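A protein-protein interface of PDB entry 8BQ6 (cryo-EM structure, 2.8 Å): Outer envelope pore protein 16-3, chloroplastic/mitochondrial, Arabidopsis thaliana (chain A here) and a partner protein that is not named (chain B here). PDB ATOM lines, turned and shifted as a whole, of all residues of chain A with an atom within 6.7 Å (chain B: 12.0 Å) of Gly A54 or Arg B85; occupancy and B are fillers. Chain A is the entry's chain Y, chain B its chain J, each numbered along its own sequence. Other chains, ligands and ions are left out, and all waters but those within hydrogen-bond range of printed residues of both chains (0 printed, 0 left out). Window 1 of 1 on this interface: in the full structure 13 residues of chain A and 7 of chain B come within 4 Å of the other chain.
Val B89 touches Thr A35 (N to CG2, 3.6 Å). Thr A39 touches Tyr B86 (CG2 to CD1, 3.8 Å). CG1 of Val A43 touches NH1 of Arg B85, at 3.3 Å. Val A50 touches Glu B82. OE2 of Glu B82 touches CB of Ala A51, 3.1 Å away. Ala A51 touches Leu B84 (CB to CB, 3.7 Å). Gly A54 touches Arg B85 (C to CB, 3.9 Å). O of Leu B84 touches CD1 of Leu A55, 3.2 Å away. Thr A58 touches Arg B85. CG2 of Thr A58 touches CG of Pro B88, 3.99 Å away.
Gly A54 touches one residue of chain B. Of chain A, only Ala A38, Thr A39, Lys A41, Val A43, Gly A54 and Thr A58 come within 4 Å of Arg B85. Ala A38 touches just one residue of chain B: Arg B85. No residue of chain B comes within 4 Å of Asp A42. Of the printed residues of chain B, Val A43 touches Arg B85. Leu A55 touches one residue of chain B. No residue of chain B comes within 4 Å of Arg A57. Of the printed residues of chain A, Leu B84 touches Ala A51 (3.7 Å) and Leu A55 (3.2 Å). Printed residues of chain A within 4 Å of Val B89: Thr A35 and Thr A39. Printed residues of chain A within 4 Å of Glu B82: Val A50 and Ala A51. Printed residues of chain B within 4 Å of Thr A58: Arg B85 and Pro B88. Printed residues of chain A within 4 Å of Pro B88: Thr A58. Arg B19 touches none of the printed residues of chain A. His B80 touches none of the printed residues of chain A. The nearest residue of chain B that does not touch Gly A54 is Leu B84 (5.9 Å). The nearest residue of chain A that does not touch Arg B85 is Leu A55 (4.1 Å). The nearest printed residue of chain A that does not touch Glu B82 is Glu A47 (5.3 Å).
The guanidinium group of Arg B85 is in hydrogen-bond range of the backbone carbonyl oxygen of Ala A38 (2.5 Å). The backbone carbonyl oxygen (O) of Thr A39 lies within hydrogen-bond range of the guanidinium group (NH2) of Arg B85. The guanidinium group of Arg B85 sits at hydrogen-bond distance from the backbone carbonyl oxygen of Lys A41 (2.7 Å).
Of the 19 printed residues of chain A, 10 touch a printed residue of chain B. Among the printed residues, 14 pairs touch across the chains.
The side-chain carboxylate of Glu B81 is in hydrogen-bond range of the side-chain hydroxyl of Tyr B86, 3.0 Å away. The guanidinium group (NH1) of Arg B85 is in hydrogen-bond range of the side-chain hydroxyl (OH) of Tyr B86, 3.2 Å away. The backbone carbonyl oxygen (O) of Tyr B86 sits at hydrogen-bond distance from the side-chain hydroxyl (OG) of Ser B90 (3.0 Å). O of Thr A35 lies within hydrogen-bond range of OG1 of Thr A39, 2.7 Å away. The side-chain carboxylate (OE2) of Glu A47 is in hydrogen-bond range of the backbone NH (N) of Gly A54. The backbone carbonyl oxygen (O) of Gly A54 sits at hydrogen-bond distance from the side-chain hydroxyl (OG1) of Thr A58 (2.9 Å).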
ATOM      1  N   THR A  35      18.927  15.905  -1.465  1.00  0.00           N
ATOM      2  CA  THR A  35      18.906  17.298  -1.907  1.00  0.00           C
ATOM      3  C   THR A  35      17.916  18.115  -1.089  1.00  0.00           C
ATOM      4  O   THR A  35      18.218  19.234  -0.656  1.00  0.00           O
ATOM      5  CB  THR A  35      18.544  17.392  -3.389  1.00  0.00           C
ATOM      6  OG1 THR A  35      19.443  16.598  -4.168  1.00  0.00           O
ATOM      7  CG2 THR A  35      18.633  18.831  -3.853  1.00  0.00           C
ATOM      8  N   LEU A  37      16.741  17.554   1.937  1.00  0.00           N
ATOM      9  CA  LEU A  37      17.214  17.713   3.308  1.00  0.00           C
ATOM     10  C   LEU A  37      18.370  18.699   3.389  1.00  0.00           C
ATOM     11  O   LEU A  37      18.467  19.480   4.340  1.00  0.00           O
ATOM     12  CB  LEU A  37      17.617  16.357   3.865  1.00  0.00           C
ATOM     13  CG  LEU A  37      16.682  15.905   4.969  1.00  0.00           C
ATOM     14  CD1 LEU A  37      15.329  15.638   4.381  1.00  0.00           C
ATOM     15  CD2 LEU A  37      17.248  14.645   5.544  1.00  0.00           C
ATOM     16  N   ALA A  38      19.271  18.665   2.409  1.00  0.00           N
ATOM     17  CA  ALA A  38      20.378  19.610   2.415  1.00  0.00           C
ATOM     18  C   ALA A  38      19.880  21.040   2.240  1.00  0.00           C
ATOM     19  O   ALA A  38      20.404  21.968   2.867  1.00  0.00           O
ATOM     20  CB  ALA A  38      21.382  19.242   1.326  1.00  0.00           C
ATOM     21  N   THR A  39      18.863  21.235   1.395  1.00  0.00           N
ATOM     22  CA  THR A  39      18.347  22.581   1.161  1.00  0.00           C
ATOM     23  C   THR A  39      17.560  23.110   2.356  1.00  0.00           C
ATOM     24  O   THR A  39      17.616  24.310   2.645  1.00  0.00           O
ATOM     25  CB  THR A  39      17.483  22.600  -0.100  1.00  0.00           C
ATOM     26  OG1 THR A  39      18.160  21.901  -1.151  1.00  0.00           O
ATOM     27  CG2 THR A  39      17.228  24.025  -0.550  1.00  0.00           C
ATOM     28  N   TRP A  40      16.831  22.239   3.062  1.00  0.00           N
ATOM     29  CA  TRP A  40      16.080  22.681   4.235  1.00  0.00           C
ATOM     30  C   TRP A  40      17.000  23.288   5.293  1.00  0.00           C
ATOM     31  O   TRP A  40      16.692  24.344   5.860  1.00  0.00           O
ATOM     32  CB  TRP A  40      15.284  21.506   4.810  1.00  0.00           C
ATOM     33  CG  TRP A  40      14.170  21.884   5.749  1.00  0.00           C
ATOM     34  CD1 TRP A  40      14.262  22.035   7.100  1.00  0.00           C
ATOM     35  CD2 TRP A  40      12.802  22.139   5.411  1.00  0.00           C
ATOM     36  NE1 TRP A  40      13.040  22.367   7.626  1.00  0.00           N
ATOM     37  CE2 TRP A  40      12.127  22.443   6.609  1.00  0.00           C
ATOM     38  CE3 TRP A  40      12.084  22.146   4.213  1.00  0.00           C
ATOM     39  CZ2 TRP A  40      10.772  22.748   6.644  1.00  0.00           C
ATOM     40  CZ3 TRP A  40      10.738  22.449   4.252  1.00  0.00           C
ATOM     41  CH2 TRP A  40      10.096  22.746   5.459  1.00  0.00           C
ATOM     42  N   LYS A  41      18.146  22.656   5.546  1.00  0.00           N
ATOM     43  CA  LYS A  41      19.081  23.085   6.582  1.00  0.00           C
ATOM     44  C   LYS A  41      19.678  24.459   6.281  1.00  0.00           C
ATOM     45  O   LYS A  41      19.887  24.842   5.128  1.00  0.00           O
ATOM     46  CB  LYS A  41      20.236  22.091   6.709  1.00  0.00           C
ATOM     47  CG  LYS A  41      19.851  20.662   7.019  1.00  0.00           C
ATOM     48  CD  LYS A  41      19.978  20.350   8.497  1.00  0.00           C
ATOM     49  CE  LYS A  41      19.047  19.220   8.893  1.00  0.00           C
ATOM     50  NZ  LYS A  41      19.742  17.918   9.065  1.00  0.00           N
ATOM     51  N   ASP A  42      19.983  25.189   7.349  1.00  0.00           N
ATOM     52  CA  ASP A  42      20.811  26.381   7.264  1.00  0.00           C
ATOM     53  C   ASP A  42      22.279  25.986   7.122  1.00  0.00           C
ATOM     54  O   ASP A  42      22.645  24.812   7.212  1.00  0.00           O
ATOM     55  CB  ASP A  42      20.619  27.256   8.499  1.00  0.00           C
ATOM     56  CG  ASP A  42      21.341  26.707   9.717  1.00  0.00           C
ATOM     57  OD1 ASP A  42      20.939  25.631  10.210  1.00  0.00           O
ATOM     58  OD2 ASP A  42      22.308  27.347  10.184  1.00  0.00           O
ATOM     59  N   VAL A  43      23.129  26.984   6.899  1.00  0.00           N
ATOM     60  CA  VAL A  43      24.565  26.735   6.795  1.00  0.00           C
ATOM     61  C   VAL A  43      25.239  27.081   8.118  1.00  0.00           C
ATOM     62  O   VAL A  43      24.827  28.033   8.798  1.00  0.00           O
ATOM     63  CB  VAL A  43      25.201  27.514   5.631  1.00  0.00           C
ATOM     64  CG1 VAL A  43      24.545  27.137   4.318  1.00  0.00           C
ATOM     65  CG2 VAL A  43      25.119  29.015   5.866  1.00  0.00           C
ATOM     66  N   GLU A  47      30.510  29.151   7.819  1.00  0.00           N
ATOM     67  CA  GLU A  47      30.402  28.851   6.395  1.00  0.00           C
ATOM     68  C   GLU A  47      29.531  29.855   5.647  1.00  0.00           C
ATOM     69  O   GLU A  47      29.331  29.704   4.436  1.00  0.00           O
ATOM     70  CB  GLU A  47      29.858  27.422   6.205  1.00  0.00           C
ATOM     71  CG  GLU A  47      30.134  26.769   4.840  1.00  0.00           C
ATOM     72  CD  GLU A  47      28.956  25.968   4.292  1.00  0.00           C
ATOM     73  OE1 GLU A  47      28.473  25.055   4.994  1.00  0.00           O
ATOM     74  OE2 GLU A  47      28.531  26.249   3.158  1.00  0.00           O
ATOM     75  N   VAL A  50      31.418  31.753   2.574  1.00  0.00           N
ATOM     76  CA  VAL A  50      32.105  30.971   1.552  1.00  0.00           C
ATOM     77  C   VAL A  50      31.144  29.913   1.019  1.00  0.00           C
ATOM     78  O   VAL A  50      30.450  29.249   1.797  1.00  0.00           O
ATOM     79  CB  VAL A  50      33.395  30.329   2.097  1.00  0.00           C
ATOM     80  CG1 VAL A  50      33.128  29.609   3.411  1.00  0.00           C
ATOM     81  CG2 VAL A  50      33.989  29.378   1.076  1.00  0.00           C
ATOM     82  N   ALA A  51      31.110  29.755  -0.306  1.00  0.00           N
ATOM     83  CA  ALA A  51      30.066  29.002  -0.993  1.00  0.00           C
ATOM     84  C   ALA A  51      30.391  27.525  -1.182  1.00  0.00           C
ATOM     85  O   ALA A  51      29.500  26.676  -1.065  1.00  0.00           O
ATOM     86  CB  ALA A  51      29.802  29.622  -2.365  1.00  0.00           C
ATOM     87  N   LEU A  52      31.643  27.213  -1.501  1.00  0.00           N
ATOM     88  CA  LEU A  52      32.007  25.865  -1.933  1.00  0.00           C
ATOM     89  C   LEU A  52      31.746  24.780  -0.891  1.00  0.00           C
ATOM     90  O   LEU A  52      31.188  23.726  -1.257  1.00  0.00           O
ATOM     91  CB  LEU A  52      33.470  25.888  -2.382  1.00  0.00           C
ATOM     92  CG  LEU A  52      34.205  24.568  -2.535  1.00  0.00           C
ATOM     93  CD1 LEU A  52      33.834  23.896  -3.845  1.00  0.00           C
ATOM     94  CD2 LEU A  52      35.695  24.826  -2.454  1.00  0.00           C
ATOM     95  N   PRO A  53      32.124  24.935   0.384  1.00  0.00           N
ATOM     96  CA  PRO A  53      31.843  23.862   1.354  1.00  0.00           C
ATOM     97  C   PRO A  53      30.363  23.540   1.504  1.00  0.00           C
ATOM     98  O   PRO A  53      30.018  22.379   1.764  1.00  0.00           O
ATOM     99  CB  PRO A  53      32.457  24.397   2.655  1.00  0.00           C
ATOM    100  CG  PRO A  53      32.582  25.861   2.458  1.00  0.00           C
ATOM    101  CD  PRO A  53      32.837  26.062   1.010  1.00  0.00           C
ATOM    102  N   GLY A  54      29.475  24.521   1.329  1.00  0.00           N
ATOM    103  CA  GLY A  54      28.050  24.219   1.337  1.00  0.00           C
ATOM    104  C   GLY A  54      27.635  23.309   0.205  1.00  0.00           C
ATOM    105  O   GLY A  54      26.835  22.388   0.395  1.00  0.00           O
ATOM    106  N   LEU A  55      28.183  23.544  -0.986  1.00  0.00           N
ATOM    107  CA  LEU A  55      27.893  22.664  -2.108  1.00  0.00           C
ATOM    108  C   LEU A  55      28.459  21.270  -1.874  1.00  0.00           C
ATOM    109  O   LEU A  55      27.824  20.266  -2.224  1.00  0.00           O
ATOM    110  CB  LEU A  55      28.446  23.260  -3.398  1.00  0.00           C
ATOM    111  CG  LEU A  55      28.187  22.401  -4.632  1.00  0.00           C
ATOM    112  CD1 LEU A  55      26.784  22.633  -5.143  1.00  0.00           C
ATOM    113  CD2 LEU A  55      29.212  22.690  -5.710  1.00  0.00           C
ATOM    114  N   ILE A  56      29.657  21.186  -1.290  1.00  0.00           N
ATOM    115  CA  ILE A  56      30.241  19.876  -1.010  1.00  0.00           C
ATOM    116  C   ILE A  56      29.364  19.106  -0.036  1.00  0.00           C
ATOM    117  O   ILE A  56      29.113  17.910  -0.212  1.00  0.00           O
ATOM    118  CB  ILE A  56      31.673  20.015  -0.469  1.00  0.00           C
ATOM    119  CG1 ILE A  56      32.585  20.656  -1.506  1.00  0.00           C
ATOM    120  CG2 ILE A  56      32.215  18.655  -0.056  1.00  0.00           C
ATOM    121  CD1 ILE A  56      33.652  21.515  -0.886  1.00  0.00           C
ATOM    122  N   ARG A  57      28.901  19.777   1.018  1.00  0.00           N
ATOM    123  CA  ARG A  57      28.045  19.110   1.992  1.00  0.00           C
ATOM    124  C   ARG A  57      26.726  18.681   1.362  1.00  0.00           C
ATOM    125  O   ARG A  57      26.211  17.598   1.664  1.00  0.00           O
ATOM    126  CB  ARG A  57      27.812  20.026   3.191  1.00  0.00           C
ATOM    127  CG  ARG A  57      26.426  19.953   3.795  1.00  0.00           C
ATOM    128  CD  ARG A  57      26.154  21.159   4.684  1.00  0.00           C
ATOM    129  NE  ARG A  57      26.994  21.163   5.875  1.00  0.00           N
ATOM    130  CZ  ARG A  57      28.117  21.857   6.006  1.00  0.00           C
ATOM    131  NH1 ARG A  57      28.556  22.650   5.042  1.00  0.00           N
ATOM    132  NH2 ARG A  57      28.818  21.750   7.131  1.00  0.00           N
ATOM    133  N   THR A  58      26.172  19.509   0.471  1.00  0.00           N
ATOM    134  CA  THR A  58      24.939  19.128  -0.212  1.00  0.00           C
ATOM    135  C   THR A  58      25.145  17.875  -1.058  1.00  0.00           C
ATOM    136  O   THR A  58      24.328  16.947  -1.027  1.00  0.00           O
ATOM    137  CB  THR A  58      24.446  20.279  -1.089  1.00  0.00           C
ATOM    138  OG1 THR A  58      24.153  21.416  -0.269  1.00  0.00           O
ATOM    139  CG2 THR A  58      23.184  19.870  -1.820  1.00  0.00           C
ATOM    140  N   LEU A  59      26.244  17.833  -1.818  1.00  0.00           N
ATOM    141  CA  LEU A  59      26.523  16.675  -2.664  1.00  0.00           C
ATOM    142  C   LEU A  59      26.822  15.434  -1.834  1.00  0.00           C
ATOM    143  O   LEU A  59      26.441  14.322  -2.212  1.00  0.00           O
ATOM    144  CB  LEU A  59      27.689  16.976  -3.599  1.00  0.00           C
ATOM    145  CG  LEU A  59      27.428  18.036  -4.663  1.00  0.00           C
ATOM    146  CD1 LEU A  59      28.732  18.455  -5.306  1.00  0.00           C
ATOM    147  CD2 LEU A  59      26.458  17.505  -5.699  1.00  0.00           C
ATOM    148  N   ARG B  19      19.008  37.658  -8.958  1.00  0.00           N
ATOM    149  CA  ARG B  19      20.366  37.369  -8.518  1.00  0.00           C
ATOM    150  C   ARG B  19      21.211  38.590  -8.187  1.00  0.00           C
ATOM    151  O   ARG B  19      22.370  38.419  -7.798  1.00  0.00           O
ATOM    152  CB  ARG B  19      21.108  36.556  -9.588  1.00  0.00           C
ATOM    153  CG  ARG B  19      20.612  35.132  -9.742  1.00  0.00           C
ATOM    154  CD  ARG B  19      21.556  34.140  -9.094  1.00  0.00           C
ATOM    155  NE  ARG B  19      21.716  34.353  -7.661  1.00  0.00           N
ATOM    156  CZ  ARG B  19      22.810  34.842  -7.096  1.00  0.00           C
ATOM    157  NH1 ARG B  19      23.841  35.247  -7.820  1.00  0.00           N
ATOM    158  NH2 ARG B  19      22.871  34.932  -5.770  1.00  0.00           N
ATOM    159  N   HIS B  80      22.490  38.934   2.350  1.00  0.00           N
ATOM    160  CA  HIS B  80      23.451  38.177   1.564  1.00  0.00           C
ATOM    161  C   HIS B  80      23.420  36.701   1.933  1.00  0.00           C
ATOM    162  O   HIS B  80      23.279  36.328   3.101  1.00  0.00           O
ATOM    163  CB  HIS B  80      24.862  38.724   1.768  1.00  0.00           C
ATOM    164  CG  HIS B  80      25.937  37.698   1.598  1.00  0.00           C
ATOM    165  ND1 HIS B  80      26.554  37.462   0.390  1.00  0.00           N
ATOM    166  CD2 HIS B  80      26.506  36.846   2.484  1.00  0.00           C
ATOM    167  CE1 HIS B  80      27.450  36.504   0.536  1.00  0.00           C
ATOM    168  NE2 HIS B  80      27.440  36.112   1.797  1.00  0.00           N
ATOM    169  N   GLU B  81      23.556  35.857   0.916  1.00  0.00           N
ATOM    170  CA  GLU B  81      23.755  34.432   1.119  1.00  0.00           C
ATOM    171  C   GLU B  81      24.375  33.844  -0.137  1.00  0.00           C
ATOM    172  O   GLU B  81      24.091  34.291  -1.253  1.00  0.00           O
ATOM    173  CB  GLU B  81      22.448  33.711   1.464  1.00  0.00           C
ATOM    174  CG  GLU B  81      21.579  33.342   0.284  1.00  0.00           C
ATOM    175  CD  GLU B  81      20.530  32.335   0.673  1.00  0.00           C
ATOM    176  OE1 GLU B  81      19.493  32.238  -0.017  1.00  0.00           O
ATOM    177  OE2 GLU B  81      20.754  31.634   1.683  1.00  0.00           O
ATOM    178  N   GLU B  82      25.243  32.861   0.065  1.00  0.00           N
ATOM    179  CA  GLU B  82      25.865  32.148  -1.038  1.00  0.00           C
ATOM    180  C   GLU B  82      24.880  31.162  -1.639  1.00  0.00           C
ATOM    181  O   GLU B  82      24.196  30.429  -0.919  1.00  0.00           O
ATOM    182  CB  GLU B  82      27.112  31.415  -0.554  1.00  0.00           C
ATOM    183  CG  GLU B  82      28.196  32.333  -0.051  1.00  0.00           C
ATOM    184  CD  GLU B  82      28.756  33.199  -1.155  1.00  0.00           C
ATOM    185  OE1 GLU B  82      28.827  34.429  -0.974  1.00  0.00           O
ATOM    186  OE2 GLU B  82      29.112  32.650  -2.216  1.00  0.00           O
ATOM    187  N   VAL B  83      24.804  31.139  -2.967  1.00  0.00           N
ATOM    188  CA  VAL B  83      23.787  30.352  -3.651  1.00  0.00           C
ATOM    189  C   VAL B  83      24.366  29.170  -4.408  1.00  0.00           C
ATOM    190  O   VAL B  83      23.637  28.534  -5.183  1.00  0.00           O
ATOM    191  CB  VAL B  83      22.940  31.231  -4.586  1.00  0.00           C
ATOM    192  CG1 VAL B  83      22.221  32.303  -3.781  1.00  0.00           C
ATOM    193  CG2 VAL B  83      23.812  31.853  -5.651  1.00  0.00           C
ATOM    194  N   LEU B  84      25.639  28.834  -4.196  1.00  0.00           N
ATOM    195  CA  LEU B  84      26.201  27.660  -4.856  1.00  0.00           C
ATOM    196  C   LEU B  84      25.527  26.379  -4.382  1.00  0.00           C
ATOM    197  O   LEU B  84      25.329  25.447  -5.168  1.00  0.00           O
ATOM    198  CB  LEU B  84      27.708  27.589  -4.620  1.00  0.00           C
ATOM    199  CG  LEU B  84      28.530  26.981  -5.757  1.00  0.00           C
ATOM    200  CD1 LEU B  84      28.451  27.844  -7.002  1.00  0.00           C
ATOM    201  CD2 LEU B  84      29.973  26.799  -5.325  1.00  0.00           C
ATOM    202  N   ARG B  85      25.157  26.315  -3.103  1.00  0.00           N
ATOM    203  CA  ARG B  85      24.549  25.105  -2.565  1.00  0.00           C
ATOM    204  C   ARG B  85      23.158  24.828  -3.122  1.00  0.00           C
ATOM    205  O   ARG B  85      22.657  23.714  -2.943  1.00  0.00           O
ATOM    206  CB  ARG B  85      24.476  25.192  -1.042  1.00  0.00           C
ATOM    207  CG  ARG B  85      23.636  26.355  -0.552  1.00  0.00           C
ATOM    208  CD  ARG B  85      23.498  26.348   0.951  1.00  0.00           C
ATOM    209  NE  ARG B  85      22.663  25.258   1.434  1.00  0.00           N
ATOM    210  CZ  ARG B  85      21.760  25.387   2.396  1.00  0.00           C
ATOM    211  NH1 ARG B  85      21.577  26.538   3.021  1.00  0.00           N
ATOM    212  NH2 ARG B  85      21.026  24.335   2.743  1.00  0.00           N
ATOM    213  N   TYR B  86      22.521  25.792  -3.784  1.00  0.00           N
ATOM    214  CA  TYR B  86      21.178  25.579  -4.308  1.00  0.00           C
ATOM    215  C   TYR B  86      21.156  25.133  -5.762  1.00  0.00           C
ATOM    216  O   TYR B  86      20.069  24.922  -6.310  1.00  0.00           O
ATOM    217  CB  TYR B  86      20.344  26.850  -4.159  1.00  0.00           C
ATOM    218  CG  TYR B  86      20.315  27.361  -2.748  1.00  0.00           C
ATOM    219  CD1 TYR B  86      19.537  26.740  -1.785  1.00  0.00           C
ATOM    220  CD2 TYR B  86      21.085  28.448  -2.373  1.00  0.00           C
ATOM    221  CE1 TYR B  86      19.516  27.196  -0.492  1.00  0.00           C
ATOM    222  CE2 TYR B  86      21.072  28.912  -1.083  1.00  0.00           C
ATOM    223  CZ  TYR B  86      20.286  28.283  -0.147  1.00  0.00           C
ATOM    224  OH  TYR B  86      20.273  28.742   1.146  1.00  0.00           O
ATOM    225  N   LEU B  87      22.315  24.995  -6.396  1.00  0.00           N
ATOM    226  CA  LEU B  87      22.370  24.511  -7.774  1.00  0.00           C
ATOM    227  C   LEU B  87      21.715  23.147  -7.975  1.00  0.00           C
ATOM    228  O   LEU B  87      21.031  22.973  -8.997  1.00  0.00           O
ATOM    229  CB  LEU B  87      23.835  24.490  -8.238  1.00  0.00           C
ATOM    230  CG  LEU B  87      24.349  25.695  -9.032  1.00  0.00           C
ATOM    231  CD1 LEU B  87      25.861  25.718  -9.008  1.00  0.00           C
ATOM    232  CD2 LEU B  87      23.854  25.654 -10.469  1.00  0.00           C
ATOM    233  N   PRO B  88      21.886  22.146  -7.092  1.00  0.00           N
ATOM    234  CA  PRO B  88      21.175  20.873  -7.297  1.00  0.00           C
ATOM    235  C   PRO B  88      19.661  20.976  -7.178  1.00  0.00           C
ATOM    236  O   PRO B  88      18.947  20.435  -8.026  1.00  0.00           O
ATOM    237  CB  PRO B  88      21.753  19.960  -6.208  1.00  0.00           C
ATOM    238  CG  PRO B  88      22.989  20.622  -5.737  1.00  0.00           C
ATOM    239  CD  PRO B  88      22.824  22.074  -5.958  1.00  0.00           C
ATOM    240  N   VAL B  89      19.150  21.631  -6.130  1.00  0.00           N
ATOM    241  CA  VAL B  89      17.699  21.720  -5.967  1.00  0.00           C
ATOM    242  C   VAL B  89      17.092  22.584  -7.064  1.00  0.00           C
ATOM    243  O   VAL B  89      16.037  22.256  -7.621  1.00  0.00           O
ATOM    244  CB  VAL B  89      17.336  22.237  -4.562  1.00  0.00           C
ATOM    245  CG1 VAL B  89      18.123  23.483  -4.220  1.00  0.00           C
ATOM    246  CG2 VAL B  89      15.847  22.505  -4.467  1.00  0.00           C
ATOM    247  N   SER B  90      17.744  23.703  -7.390  1.00  0.00           N
ATOM    248  CA  SER B  90      17.306  24.470  -8.547  1.00  0.00           C
ATOM    249  C   SER B  90      17.350  23.616  -9.801  1.00  0.00           C
ATOM    250  O   SER B  90      16.441  23.690 -10.625  1.00  0.00           O
ATOM    251  CB  SER B  90      18.174  25.708  -8.738  1.00  0.00           C
ATOM    252  OG  SER B  90      19.458  25.337  -9.202  1.00  0.00           O
ATOM    253  N   GLY B  91      18.383  22.783  -9.942  1.00  0.00           N
ATOM    254  CA  GLY B  91      18.478  21.937 -11.118  1.00  0.00           C
ATOM    255  C   GLY B  91      17.313  20.973 -11.240  1.00  0.00           C
ATOM    256  O   GLY B  91      16.675  20.890 -12.289  1.00  0.00           O
ATOM    257  N   ILE B  92      16.997  20.258 -10.160  1.00  0.00           N
ATOM    258  CA  ILE B  92      15.903  19.292 -10.219  1.00  0.00           C
ATOM    259  C   ILE B  92      14.568  19.998 -10.430  1.00  0.00           C
ATOM    260  O   ILE B  92      13.779  19.612 -11.302  1.00  0.00           O
ATOM    261  CB  ILE B  92      15.883  18.406  -8.962  1.00  0.00           C
ATOM    262  CG1 ILE B  92      17.017  17.379  -9.013  1.00  0.00           C
ATOM    263  CG2 ILE B  92      14.544  17.723  -8.818  1.00  0.00           C
ATOM    264  CD1 ILE B  92      17.874  17.354  -7.781  1.00  0.00           C
ATOM    265  N   ILE B  93      14.287  21.037  -9.639  1.00  0.00           N
ATOM    266  CA  ILE B  93      12.998  21.713  -9.768  1.00  0.00           C
ATOM    267  C   ILE B  93      12.852  22.310 -11.160  1.00  0.00           C
ATOM    268  O   ILE B  93      11.842  22.093 -11.846  1.00  0.00           O
ATOM    269  CB  ILE B  93      12.842  22.788  -8.676  1.00  0.00           C
ATOM    270  CG1 ILE B  93      12.903  22.149  -7.289  1.00  0.00           C
ATOM    271  CG2 ILE B  93      11.533  23.538  -8.855  1.00  0.00           C
ATOM    272  CD1 ILE B  93      11.740  21.254  -6.990  1.00  0.00           C
